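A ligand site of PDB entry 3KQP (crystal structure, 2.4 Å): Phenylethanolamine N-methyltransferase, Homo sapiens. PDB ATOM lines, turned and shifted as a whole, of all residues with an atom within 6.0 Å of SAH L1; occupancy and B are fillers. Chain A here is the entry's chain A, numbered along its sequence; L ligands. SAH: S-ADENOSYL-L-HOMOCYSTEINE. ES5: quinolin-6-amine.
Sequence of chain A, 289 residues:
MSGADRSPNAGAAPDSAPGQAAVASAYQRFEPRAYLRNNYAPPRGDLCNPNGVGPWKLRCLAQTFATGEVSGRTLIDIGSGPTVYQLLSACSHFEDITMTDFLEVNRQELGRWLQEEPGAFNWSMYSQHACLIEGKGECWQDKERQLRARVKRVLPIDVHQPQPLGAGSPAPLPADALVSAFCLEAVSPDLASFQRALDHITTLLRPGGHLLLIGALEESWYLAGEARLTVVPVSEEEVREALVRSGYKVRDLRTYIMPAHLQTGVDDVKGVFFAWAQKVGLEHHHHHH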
ATOM      1  N   ALA A  24       0.705  -5.373  33.847  1.00  0.00           N
ATOM      2  CA  ALA A  24       0.369  -6.365  32.831  1.00  0.00           C
ATOM      3  C   ALA A  24      -0.351  -5.724  31.646  1.00  0.00           C
ATOM      4  O   ALA A  24       0.056  -5.885  30.492  1.00  0.00           O
ATOM      5  CB  ALA A  24      -0.484  -7.476  33.435  1.00  0.00           C
ATOM      6  N   TYR A  27       0.634  -4.616  28.065  1.00  0.00           N
ATOM      7  CA  TYR A  27       0.867  -5.456  26.890  1.00  0.00           C
ATOM      8  C   TYR A  27      -0.211  -5.344  25.818  1.00  0.00           C
ATOM      9  O   TYR A  27      -0.061  -5.905  24.735  1.00  0.00           O
ATOM     10  CB  TYR A  27       1.097  -6.929  27.275  1.00  0.00           C
ATOM     11  CG  TYR A  27       2.543  -7.194  27.604  1.00  0.00           C
ATOM     12  CD1 TYR A  27       2.983  -7.208  28.926  1.00  0.00           C
ATOM     13  CD2 TYR A  27       3.482  -7.365  26.600  1.00  0.00           C
ATOM     14  CE1 TYR A  27       4.314  -7.426  29.222  1.00  0.00           C
ATOM     15  CE2 TYR A  27       4.813  -7.576  26.883  1.00  0.00           C
ATOM     16  CZ  TYR A  27       5.226  -7.603  28.192  1.00  0.00           C
ATOM     17  OH  TYR A  27       6.546  -7.805  28.481  1.00  0.00           O
ATOM     18  N   PHE A  30       1.160  -3.256  23.030  1.00  0.00           N
ATOM     19  CA  PHE A  30       2.351  -3.860  22.443  1.00  0.00           C
ATOM     20  C   PHE A  30       2.210  -3.956  20.929  1.00  0.00           C
ATOM     21  O   PHE A  30       1.337  -4.668  20.435  1.00  0.00           O
ATOM     22  CB  PHE A  30       2.560  -5.239  23.045  1.00  0.00           C
ATOM     23  CG  PHE A  30       3.801  -5.941  22.588  1.00  0.00           C
ATOM     24  CD1 PHE A  30       4.908  -6.021  23.419  1.00  0.00           C
ATOM     25  CD2 PHE A  30       3.853  -6.571  21.346  1.00  0.00           C
ATOM     26  CE1 PHE A  30       6.042  -6.699  23.028  1.00  0.00           C
ATOM     27  CE2 PHE A  30       4.987  -7.243  20.942  1.00  0.00           C
ATOM     28  CZ  PHE A  30       6.090  -7.307  21.782  1.00  0.00           C
ATOM     29  N   TYR A  35       8.447  -3.834  17.982  1.00  0.00           N
ATOM     30  CA  TYR A  35       9.354  -4.681  18.733  1.00  0.00           C
ATOM     31  C   TYR A  35      10.379  -5.391  17.829  1.00  0.00           C
ATOM     32  O   TYR A  35      11.564  -5.453  18.165  1.00  0.00           O
ATOM     33  CB  TYR A  35       8.574  -5.694  19.559  1.00  0.00           C
ATOM     34  CG  TYR A  35       9.430  -6.723  20.259  1.00  0.00           C
ATOM     35  CD1 TYR A  35      10.127  -6.406  21.427  1.00  0.00           C
ATOM     36  CD2 TYR A  35       9.544  -8.022  19.762  1.00  0.00           C
ATOM     37  CE1 TYR A  35      10.910  -7.344  22.066  1.00  0.00           C
ATOM     38  CE2 TYR A  35      10.320  -8.966  20.398  1.00  0.00           C
ATOM     39  CZ  TYR A  35      10.994  -8.633  21.551  1.00  0.00           C
ATOM     40  OH  TYR A  35      11.758  -9.577  22.181  1.00  0.00           O
ATOM     41  N   TYR A  40      15.336  -6.794  16.188  1.00  0.00           N
ATOM     42  CA  TYR A  40      15.742  -7.786  15.204  1.00  0.00           C
ATOM     43  C   TYR A  40      16.055  -7.192  13.837  1.00  0.00           C
ATOM     44  O   TYR A  40      16.426  -7.912  12.915  1.00  0.00           O
ATOM     45  CB  TYR A  40      14.709  -8.923  15.144  1.00  0.00           C
ATOM     46  CG  TYR A  40      14.639  -9.641  16.474  1.00  0.00           C
ATOM     47  CD1 TYR A  40      13.680  -9.299  17.424  1.00  0.00           C
ATOM     48  CD2 TYR A  40      15.586 -10.587  16.814  1.00  0.00           C
ATOM     49  CE1 TYR A  40      13.645  -9.933  18.660  1.00  0.00           C
ATOM     50  CE2 TYR A  40      15.568 -11.217  18.035  1.00  0.00           C
ATOM     51  CZ  TYR A  40      14.597 -10.898  18.958  1.00  0.00           C
ATOM     52  OH  TYR A  40      14.599 -11.545  20.170  1.00  0.00           O
ATOM     53  N   LYS A  57      23.194 -15.098  20.735  1.00  0.00           N
ATOM     54  CA  LYS A  57      21.981 -15.866  21.001  1.00  0.00           C
ATOM     55  C   LYS A  57      21.869 -17.118  20.125  1.00  0.00           C
ATOM     56  O   LYS A  57      21.646 -18.223  20.644  1.00  0.00           O
ATOM     57  CB  LYS A  57      20.738 -14.994  20.853  1.00  0.00           C
ATOM     58  CG  LYS A  57      20.747 -13.789  21.805  1.00  0.00           C
ATOM     59  CD  LYS A  57      19.353 -13.204  22.036  1.00  0.00           C
ATOM     60  CE  LYS A  57      18.710 -12.736  20.742  1.00  0.00           C
ATOM     61  NZ  LYS A  57      17.345 -12.192  20.958  1.00  0.00           N
ATOM     62  N   ASP A  77       7.580 -23.539  22.841  1.00  0.00           N
ATOM     63  CA  ASP A  77       8.250 -22.253  22.996  1.00  0.00           C
ATOM     64  C   ASP A  77       7.345 -21.328  23.789  1.00  0.00           C
ATOM     65  O   ASP A  77       6.208 -21.055  23.385  1.00  0.00           O
ATOM     66  CB  ASP A  77       8.585 -21.662  21.619  1.00  0.00           C
ATOM     67  CG  ASP A  77       9.335 -20.346  21.722  1.00  0.00           C
ATOM     68  OD1 ASP A  77      10.026 -20.124  22.738  1.00  0.00           O
ATOM     69  OD2 ASP A  77       9.261 -19.539  20.771  1.00  0.00           O
ATOM     70  N   ILE A  78       7.840 -20.875  24.935  1.00  0.00           N
ATOM     71  CA  ILE A  78       7.056 -20.055  25.874  1.00  0.00           C
ATOM     72  C   ILE A  78       7.197 -18.563  25.582  1.00  0.00           C
ATOM     73  O   ILE A  78       8.294 -18.017  25.670  1.00  0.00           O
ATOM     74  CB  ILE A  78       7.504 -20.283  27.341  1.00  0.00           C
ATOM     75  CG1 ILE A  78       7.596 -21.786  27.679  1.00  0.00           C
ATOM     76  CG2 ILE A  78       6.584 -19.546  28.309  1.00  0.00           C
ATOM     77  CD1 ILE A  78       6.313 -22.545  27.484  1.00  0.00           C
ATOM     78  N   GLY A  79       6.080 -17.916  25.257  1.00  0.00           N
ATOM     79  CA  GLY A  79       6.091 -16.484  25.029  1.00  0.00           C
ATOM     80  C   GLY A  79       6.853 -16.143  23.763  1.00  0.00           C
ATOM     81  O   GLY A  79       7.745 -15.292  23.771  1.00  0.00           O
ATOM     82  N   SER A  80       6.501 -16.824  22.676  1.00  0.00           N
ATOM     83  CA  SER A  80       7.178 -16.681  21.401  1.00  0.00           C
ATOM     84  C   SER A  80       7.236 -15.257  20.879  1.00  0.00           C
ATOM     85  O   SER A  80       8.178 -14.884  20.162  1.00  0.00           O
ATOM     86  CB  SER A  80       6.494 -17.577  20.357  1.00  0.00           C
ATOM     87  OG  SER A  80       6.488 -18.926  20.794  1.00  0.00           O
ATOM     88  N   GLY A  81       6.237 -14.448  21.236  1.00  0.00           N
ATOM     89  CA  GLY A  81       6.061 -13.153  20.605  1.00  0.00           C
ATOM     90  C   GLY A  81       5.964 -13.311  19.089  1.00  0.00           C
ATOM     91  O   GLY A  81       5.430 -14.313  18.595  1.00  0.00           O
ATOM     92  N   PRO A  82       6.486 -12.333  18.346  1.00  0.00           N
ATOM     93  CA  PRO A  82       6.414 -12.392  16.887  1.00  0.00           C
ATOM     94  C   PRO A  82       7.718 -12.931  16.296  1.00  0.00           C
ATOM     95  O   PRO A  82       8.012 -12.649  15.151  1.00  0.00           O
ATOM     96  CB  PRO A  82       6.266 -10.914  16.500  1.00  0.00           C
ATOM     97  CG  PRO A  82       6.817 -10.121  17.713  1.00  0.00           C
ATOM     98  CD  PRO A  82       7.181 -11.112  18.785  1.00  0.00           C
ATOM     99  N   THR A  83       8.497 -13.667  17.078  1.00  0.00           N
ATOM    100  CA  THR A  83       9.818 -14.093  16.607  1.00  0.00           C
ATOM    101  C   THR A  83       9.957 -15.616  16.470  1.00  0.00           C
ATOM    102  O   THR A  83       9.344 -16.367  17.239  1.00  0.00           O
ATOM    103  CB  THR A  83      10.966 -13.492  17.468  1.00  0.00           C
ATOM    104  OG1 THR A  83      11.148 -14.239  18.674  1.00  0.00           O
ATOM    105  CG2 THR A  83      10.691 -12.026  17.813  1.00  0.00           C
ATOM    106  N   TYR A  85      13.305 -16.978  15.444  1.00  0.00           N
ATOM    107  CA  TYR A  85      14.750 -17.260  15.478  1.00  0.00           C
ATOM    108  C   TYR A  85      15.091 -18.262  16.561  1.00  0.00           C
ATOM    109  O   TYR A  85      16.003 -19.070  16.408  1.00  0.00           O
ATOM    110  CB  TYR A  85      15.546 -15.977  15.712  1.00  0.00           C
ATOM    111  CG  TYR A  85      15.454 -15.487  17.155  1.00  0.00           C
ATOM    112  CD1 TYR A  85      16.394 -15.869  18.095  1.00  0.00           C
ATOM    113  CD2 TYR A  85      14.420 -14.663  17.560  1.00  0.00           C
ATOM    114  CE1 TYR A  85      16.309 -15.437  19.411  1.00  0.00           C
ATOM    115  CE2 TYR A  85      14.330 -14.224  18.873  1.00  0.00           C
ATOM    116  CZ  TYR A  85      15.273 -14.614  19.792  1.00  0.00           C
ATOM    117  OH  TYR A  85      15.190 -14.191  21.088  1.00  0.00           O
ATOM    118  N   GLN A  86      14.369 -18.195  17.684  1.00  0.00           N
ATOM    119  CA  GLN A  86      14.721 -19.000  18.851  1.00  0.00           C
ATOM    120  C   GLN A  86      14.480 -20.490  18.632  1.00  0.00           C
ATOM    121  O   GLN A  86      14.841 -21.295  19.473  1.00  0.00           O
ATOM    122  CB  GLN A  86      14.005 -18.511  20.119  1.00  0.00           C
ATOM    123  CG  GLN A  86      12.481 -18.680  20.144  1.00  0.00           C
ATOM    124  CD  GLN A  86      11.739 -17.494  19.542  1.00  0.00           C
ATOM    125  OE1 GLN A  86      12.321 -16.711  18.776  1.00  0.00           O
ATOM    126  NE2 GLN A  86      10.452 -17.359  19.862  1.00  0.00           N
ATOM    127  N   ASP A 101       1.887 -17.415  22.671  1.00  0.00           N
ATOM    128  CA  ASP A 101       1.990 -16.061  23.210  1.00  0.00           C
ATOM    129  C   ASP A 101       0.680 -15.591  23.830  1.00  0.00           C
ATOM    130  O   ASP A 101      -0.398 -16.070  23.482  1.00  0.00           O
ATOM    131  CB  ASP A 101       2.466 -15.061  22.154  1.00  0.00           C
ATOM    132  CG  ASP A 101       3.080 -13.819  22.775  1.00  0.00           C
ATOM    133  OD1 ASP A 101       4.162 -13.951  23.407  1.00  0.00           O
ATOM    134  OD2 ASP A 101       2.481 -12.729  22.650  1.00  0.00           O
ATOM    135  N   PHE A 102       0.806 -14.631  24.738  1.00  0.00           N
ATOM    136  CA  PHE A 102      -0.334 -14.061  25.448  1.00  0.00           C
ATOM    137  C   PHE A 102      -1.175 -13.176  24.522  1.00  0.00           C
ATOM    138  O   PHE A 102      -2.392 -13.074  24.679  1.00  0.00           O
ATOM    139  CB  PHE A 102       0.176 -13.270  26.663  1.00  0.00           C
ATOM    140  CG  PHE A 102      -0.897 -12.534  27.423  1.00  0.00           C
ATOM    141  CD1 PHE A 102      -1.652 -13.187  28.377  1.00  0.00           C
ATOM    142  CD2 PHE A 102      -1.114 -11.196  27.199  1.00  0.00           C
ATOM    143  CE1 PHE A 102      -2.645 -12.513  29.085  1.00  0.00           C
ATOM    144  CE2 PHE A 102      -2.098 -10.502  27.909  1.00  0.00           C
ATOM    145  CZ  PHE A 102      -2.857 -11.176  28.852  1.00  0.00           C
ATOM    146  N   LEU A 103      -0.521 -12.557  23.541  1.00  0.00           N
ATOM    147  CA  LEU A 103      -1.179 -11.629  22.628  1.00  0.00           C
ATOM    148  C   LEU A 103      -1.577 -12.254  21.293  1.00  0.00           C
ATOM    149  O   LEU A 103      -0.797 -12.956  20.645  1.00  0.00           O
ATOM    150  CB  LEU A 103      -0.300 -10.399  22.377  1.00  0.00           C
ATOM    151  CG  LEU A 103      -0.012  -9.477  23.559  1.00  0.00           C
ATOM    152  CD1 LEU A 103       1.077  -8.480  23.186  1.00  0.00           C
ATOM    153  CD2 LEU A 103      -1.285  -8.764  24.032  1.00  0.00           C
ATOM    154  N   ASN A 106       0.549 -10.962  18.256  1.00  0.00           N
ATOM    155  CA  ASN A 106       1.772 -11.738  18.072  1.00  0.00           C
ATOM    156  C   ASN A 106       1.525 -13.064  17.373  1.00  0.00           C
ATOM    157  O   ASN A 106       2.263 -13.427  16.455  1.00  0.00           O
ATOM    158  CB  ASN A 106       2.467 -11.974  19.410  1.00  0.00           C
ATOM    159  CG  ASN A 106       3.399 -10.850  19.771  1.00  0.00           C
ATOM    160  OD1 ASN A 106       3.907 -10.785  20.892  1.00  0.00           O
ATOM    161  ND2 ASN A 106       3.646  -9.959  18.823  1.00  0.00           N
ATOM    162  N   ILE A 157      -1.491 -18.282  25.817  1.00  0.00           N
ATOM    163  CA  ILE A 157      -0.767 -18.739  26.993  1.00  0.00           C
ATOM    164  C   ILE A 157      -0.603 -17.586  27.966  1.00  0.00           C
ATOM    165  O   ILE A 157      -0.418 -16.434  27.569  1.00  0.00           O
ATOM    166  CB  ILE A 157       0.631 -19.290  26.613  1.00  0.00           C
ATOM    167  CG1 ILE A 157       1.294 -19.944  27.826  1.00  0.00           C
ATOM    168  CG2 ILE A 157       1.505 -18.186  26.043  1.00  0.00           C
ATOM    169  CD1 ILE A 157       2.655 -20.536  27.522  1.00  0.00           C
ATOM    170  N   ASP A 158      -0.685 -17.905  29.263  1.00  0.00           N
ATOM    171  CA  ASP A 158      -0.469 -16.925  30.319  1.00  0.00           C
ATOM    172  C   ASP A 158       0.300 -17.589  31.442  1.00  0.00           C
ATOM    173  O   ASP A 158      -0.255 -18.407  32.181  1.00  0.00           O
ATOM    174  CB  ASP A 158      -1.792 -16.381  30.843  1.00  0.00           C
ATOM    175  CG  ASP A 158      -1.608 -15.406  31.986  1.00  0.00           C
ATOM    176  OD1 ASP A 158      -0.474 -15.315  32.514  1.00  0.00           O
ATOM    177  OD2 ASP A 158      -2.578 -14.719  32.374  1.00  0.00           O
ATOM    178  N   VAL A 159       1.574 -17.231  31.590  1.00  0.00           N
ATOM    179  CA  VAL A 159       2.441 -17.896  32.548  1.00  0.00           C
ATOM    180  C   VAL A 159       2.091 -17.546  33.995  1.00  0.00           C
ATOM    181  O   VAL A 159       2.544 -18.213  34.926  1.00  0.00           O
ATOM    182  CB  VAL A 159       3.921 -17.595  32.267  1.00  0.00           C
ATOM    183  CG1 VAL A 159       4.289 -18.030  30.862  1.00  0.00           C
ATOM    184  CG2 VAL A 159       4.206 -16.111  32.464  1.00  0.00           C
ATOM    185  N   HIS A 160       1.288 -16.499  34.177  1.00  0.00           N
ATOM    186  CA  HIS A 160       0.800 -16.161  35.506  1.00  0.00           C
ATOM    187  C   HIS A 160      -0.203 -17.220  35.978  1.00  0.00           C
ATOM    188  O   HIS A 160      -0.483 -17.337  37.166  1.00  0.00           O
ATOM    189  CB  HIS A 160       0.166 -14.774  35.520  1.00  0.00           C
ATOM    190  CG  HIS A 160       1.098 -13.681  35.108  1.00  0.00           C
ATOM    191  ND1 HIS A 160       2.380 -13.581  35.601  1.00  0.00           N
ATOM    192  CD2 HIS A 160       0.936 -12.643  34.265  1.00  0.00           C
ATOM    193  CE1 HIS A 160       2.981 -12.536  35.064  1.00  0.00           C
ATOM    194  NE2 HIS A 160       2.122 -11.943  34.244  1.00  0.00           N
ATOM    195  N   SER A 180      12.220 -20.627  26.112  1.00  0.00           N
ATOM    196  CA  SER A 180      11.588 -19.358  26.415  1.00  0.00           C
ATOM    197  C   SER A 180      12.610 -18.238  26.403  1.00  0.00           C
ATOM    198  O   SER A 180      13.632 -18.302  27.096  1.00  0.00           O
ATOM    199  CB  SER A 180      10.877 -19.378  27.771  1.00  0.00           C
ATOM    200  OG  SER A 180      10.120 -18.200  27.962  1.00  0.00           O
ATOM    201  N   ALA A 181      12.331 -17.211  25.624  1.00  0.00           N
ATOM    202  CA  ALA A 181      13.273 -16.133  25.459  1.00  0.00           C
ATOM    203  C   ALA A 181      12.620 -14.786  25.708  1.00  0.00           C
ATOM    204  O   ALA A 181      11.660 -14.422  25.022  1.00  0.00           O
ATOM    205  CB  ALA A 181      13.889 -16.176  24.060  1.00  0.00           C
ATOM    206  N   PHE A 182      13.141 -14.074  26.698  1.00  0.00           N
ATOM    207  CA  PHE A 182      12.712 -12.708  26.984  1.00  0.00           C
ATOM    208  C   PHE A 182      11.238 -12.606  27.345  1.00  0.00           C
ATOM    209  O   PHE A 182      10.602 -11.572  27.161  1.00  0.00           O
ATOM    210  CB  PHE A 182      13.085 -11.781  25.825  1.00  0.00           C
ATOM    211  CG  PHE A 182      14.540 -11.846  25.461  1.00  0.00           C
ATOM    212  CD1 PHE A 182      14.974 -12.659  24.424  1.00  0.00           C
ATOM    213  CD2 PHE A 182      15.488 -11.115  26.176  1.00  0.00           C
ATOM    214  CE1 PHE A 182      16.320 -12.730  24.094  1.00  0.00           C
ATOM    215  CE2 PHE A 182      16.825 -11.185  25.863  1.00  0.00           C
ATOM    216  CZ  PHE A 182      17.251 -11.997  24.811  1.00  0.00           C
ATOM    217  N   CYS A 183      10.686 -13.685  27.878  1.00  0.00           N
ATOM    218  CA  CYS A 183       9.317 -13.665  28.374  1.00  0.00           C
ATOM    219  C   CYS A 183       9.257 -13.396  29.884  1.00  0.00           C
ATOM    220  O   CYS A 183       8.887 -12.293  30.303  1.00  0.00           O
ATOM    221  CB  CYS A 183       8.617 -14.979  28.047  1.00  0.00           C
ATOM    222  SG  CYS A 183       6.873 -15.038  28.523  1.00  0.00           S
ATOM    223  N   ALA A 186      10.148 -10.252  31.594  1.00  0.00           N
ATOM    224  CA  ALA A 186       9.387  -9.204  30.931  1.00  0.00           C
ATOM    225  C   ALA A 186       7.887  -9.206  31.279  1.00  0.00           C
ATOM    226  O   ALA A 186       7.160  -8.304  30.858  1.00  0.00           O
ATOM    227  CB  ALA A 186       9.582  -9.276  29.412  1.00  0.00           C
ATOM    228  N   VAL A 187       7.438 -10.214  32.019  1.00  0.00           N
ATOM    229  CA  VAL A 187       6.027 -10.271  32.446  1.00  0.00           C
ATOM    230  C   VAL A 187       5.888 -10.277  33.970  1.00  0.00           C
ATOM    231  O   VAL A 187       4.800 -10.481  34.495  1.00  0.00           O
ATOM    232  CB  VAL A 187       5.286 -11.482  31.855  1.00  0.00           C
ATOM    233  CG1 VAL A 187       5.290 -11.439  30.333  1.00  0.00           C
ATOM    234  CG2 VAL A 187       5.896 -12.786  32.355  1.00  0.00           C
ATOM    235  N   TYR A 222      11.289  -1.899  28.628  1.00  0.00           N
ATOM    236  CA  TYR A 222      11.562  -1.847  27.193  1.00  0.00           C
ATOM    237  C   TYR A 222      10.327  -1.375  26.449  1.00  0.00           C
ATOM    238  O   TYR A 222       9.219  -1.449  26.971  1.00  0.00           O
ATOM    239  CB  TYR A 222      12.051  -3.192  26.651  1.00  0.00           C
ATOM    240  CG  TYR A 222      10.982  -4.246  26.493  1.00  0.00           C
ATOM    241  CD1 TYR A 222      10.438  -4.521  25.243  1.00  0.00           C
ATOM    242  CD2 TYR A 222      10.524  -4.989  27.584  1.00  0.00           C
ATOM    243  CE1 TYR A 222       9.478  -5.488  25.075  1.00  0.00           C
ATOM    244  CE2 TYR A 222       9.558  -5.969  27.426  1.00  0.00           C
ATOM    245  CZ  TYR A 222       9.029  -6.211  26.168  1.00  0.00           C
ATOM    246  OH  TYR A 222       8.066  -7.179  25.977  1.00  0.00           O
HETATM  247  N   SAH L   1      10.217 -14.914  22.562  1.00  0.00           N
HETATM  248  CA  SAH L   1      10.378 -13.559  22.047  1.00  0.00           C
HETATM  249  CB  SAH L   1      10.107 -12.594  23.209  1.00  0.00           C
HETATM  250  CG  SAH L   1       8.841 -11.771  22.919  1.00  0.00           C
HETATM  251  SD  SAH L   1       8.828 -10.406  24.113  1.00  0.00           S
HETATM  252  C   SAH L   1      11.838 -13.359  21.596  1.00  0.00           C
HETATM  253  O   SAH L   1      12.667 -14.151  21.910  1.00  0.00           O
HETATM  254  OXT SAH L   1      12.241 -12.065  21.252  1.00  0.00           O
HETATM  255  C5' SAH L   1       7.921 -10.908  25.606  1.00  0.00           C
HETATM  256  C4' SAH L   1       6.687 -11.735  25.206  1.00  0.00           C
HETATM  257  O4' SAH L   1       5.947 -12.154  26.391  1.00  0.00           O
HETATM  258  C3' SAH L   1       5.701 -10.931  24.327  1.00  0.00           C
HETATM  259  O3' SAH L   1       5.405 -11.651  23.161  1.00  0.00           O
HETATM  260  C2' SAH L   1       4.493 -10.834  25.219  1.00  0.00           C
HETATM  261  O2' SAH L   1       3.265 -10.623  24.557  1.00  0.00           O
HETATM  262  C1' SAH L   1       4.547 -12.150  25.982  1.00  0.00           C
HETATM  263  N9  SAH L   1       3.706 -12.051  27.150  1.00  0.00           N
HETATM  264  C8  SAH L   1       3.159 -10.789  27.740  1.00  0.00           C
HETATM  265  N7  SAH L   1       2.396 -11.149  28.916  1.00  0.00           N
HETATM  266  C5  SAH L   1       2.467 -12.609  29.078  1.00  0.00           C
HETATM  267  C6  SAH L   1       1.871 -13.518  30.115  1.00  0.00           C
HETATM  268  N6  SAH L   1       1.085 -12.946  31.197  1.00  0.00           N
HETATM  269  N1  SAH L   1       2.114 -14.957  30.024  1.00  0.00           N
HETATM  270  C2  SAH L   1       2.944 -15.529  28.907  1.00  0.00           C
HETATM  271  N3  SAH L   1       3.522 -14.618  27.872  1.00  0.00           N
HETATM  272  C4  SAH L   1       3.281 -13.171  27.975  1.00  0.00           C
HETATM  273  C10 ES5 L   2      16.895  -7.751  24.152  1.00  0.00           C
HETATM  274  N01 ES5 L   2      13.569  -6.733  25.678  1.00  0.00           N
HETATM  275  C02 ES5 L   2      14.572  -7.440  24.888  1.00  0.00           C
HETATM  276  C03 ES5 L   2      14.182  -8.555  24.097  1.00  0.00           C
HETATM  277  C04 ES5 L   2      15.141  -9.257  23.329  1.00  0.00           C
HETATM  278  C05 ES5 L   2      16.508  -8.858  23.374  1.00  0.00           C
HETATM  279  N06 ES5 L   2      17.448  -9.549  22.628  1.00  0.00           N
HETATM  280  C07 ES5 L   2      18.771  -9.161  22.662  1.00  0.00           C
HETATM  281  C08 ES5 L   2      19.176  -8.056  23.438  1.00  0.00           C
HETATM  282  C09 ES5 L   2      18.231  -7.358  24.181  1.00  0.00           C
HETATM  283  C11 ES5 L   2      15.931  -7.042  24.917  1.00  0.00           C
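The backbone NH of Ile 157 sits at hydrogen-bond distance from the backbone carbonyl oxygen of Asp 101, 3.4 Å away. NE2 of His 160 sits close to O of Val 187. OH of Tyr 40 sits at hydrogen-bond distance from NZ of Lys 57 (2.9 Å). The backbone NH (N) of Gly 81 lies within hydrogen-bond range of the side-chain carboxylate (OD1) of Asp 101. The side-chain carboxylate (OD2) of Asp 77 lies within hydrogen-bond range of the side-chain hydroxyl (OG) of Ser 80. The side-chain carboxylate (OD1) of Asp 158 is in hydrogen-bond range of the backbone NH (N) of His 160 (2.7 Å). The side-chain hydroxyl (OH) of Tyr 85 sits at hydrogen-bond distance from the side-chain hydroxyl (OH) of Tyr 40 (2.9 Å). OH of Tyr 85 lies within hydrogen-bond range of NZ of Lys 57.
An oxygen (OXT) of SAH L1 lies within hydrogen-bond range of the side-chain hydroxyl (OH) of Tyr 40, 2.6 Å away. NZ of Lys 57 is in hydrogen-bond range of N06 of ES5 L2, 3.1 Å away. The backbone NH of Gly 81 lies close to an oxygen (O3') of SAH L1 (3.5 Å). O of Ala 181 is in hydrogen-bond range of N of SAH L1, 2.9 Å away. A nitrogen (N6) of SAH L1 sits close to a ring nitrogen (NE2) of His 160. The side-chain carboxylate (OD1) of Asp 101 lies within hydrogen-bond range of an oxygen (O3') of SAH L1. An oxygen (O) of SAH L1 is in hydrogen-bond range of the side-chain hydroxyl (OH) of Tyr 85 (2.7 Å). The backbone carbonyl oxygen (O) of Gly 79 lies within hydrogen-bond range of a nitrogen (N) of SAH L1. The side-chain carboxylate of Asp 158 is in hydrogen-bond range of a nitrogen (N6) of SAH L1 (3.1 Å). The side-chain amide oxygen (OD1) of Asn 106 sits at hydrogen-bond distance from an oxygen (O3') of SAH L1. N of Val 159 lies within hydrogen-bond range of N1 of SAH L1 (2.8 Å). The backbone carbonyl oxygen of Ser 80 sits at hydrogen-bond distance from a nitrogen (N) of SAH L1, 3.1 Å away. The side-chain hydroxyl of Tyr 35 sits at hydrogen-bond distance from an oxygen (OXT) of SAH L1, at 2.7 Å. The side-chain sulfur of Cys 183 sits at hydrogen-bond distance from a nitrogen (N3) of SAH L1 (3.4 Å).
O of Phe 182 lies close to SD of SAH L1, at 3.7 Å. Merely in contact with SAH L1: Tyr 27 (3.6 Å), Thr 83 (3.1 Å), Gln 86 (3.7 Å), Phe 102 (3.4 Å), Leu 103 (3.4 Å), Ile 157 (3.7 Å), Val 187 (3.2 Å) and Tyr 222 (3.8 Å). Hydrophobic or aromatic side chains within 4 Å of SAH L1: Tyr 27, Tyr 35, Tyr 40, Tyr 85, Phe 102, Leu 103, Val 159, His 160, Ala 181, Phe 182 and Val 187. The nearest printed residue that does not touch SAH L1 is Phe 30 (4.4 Å).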
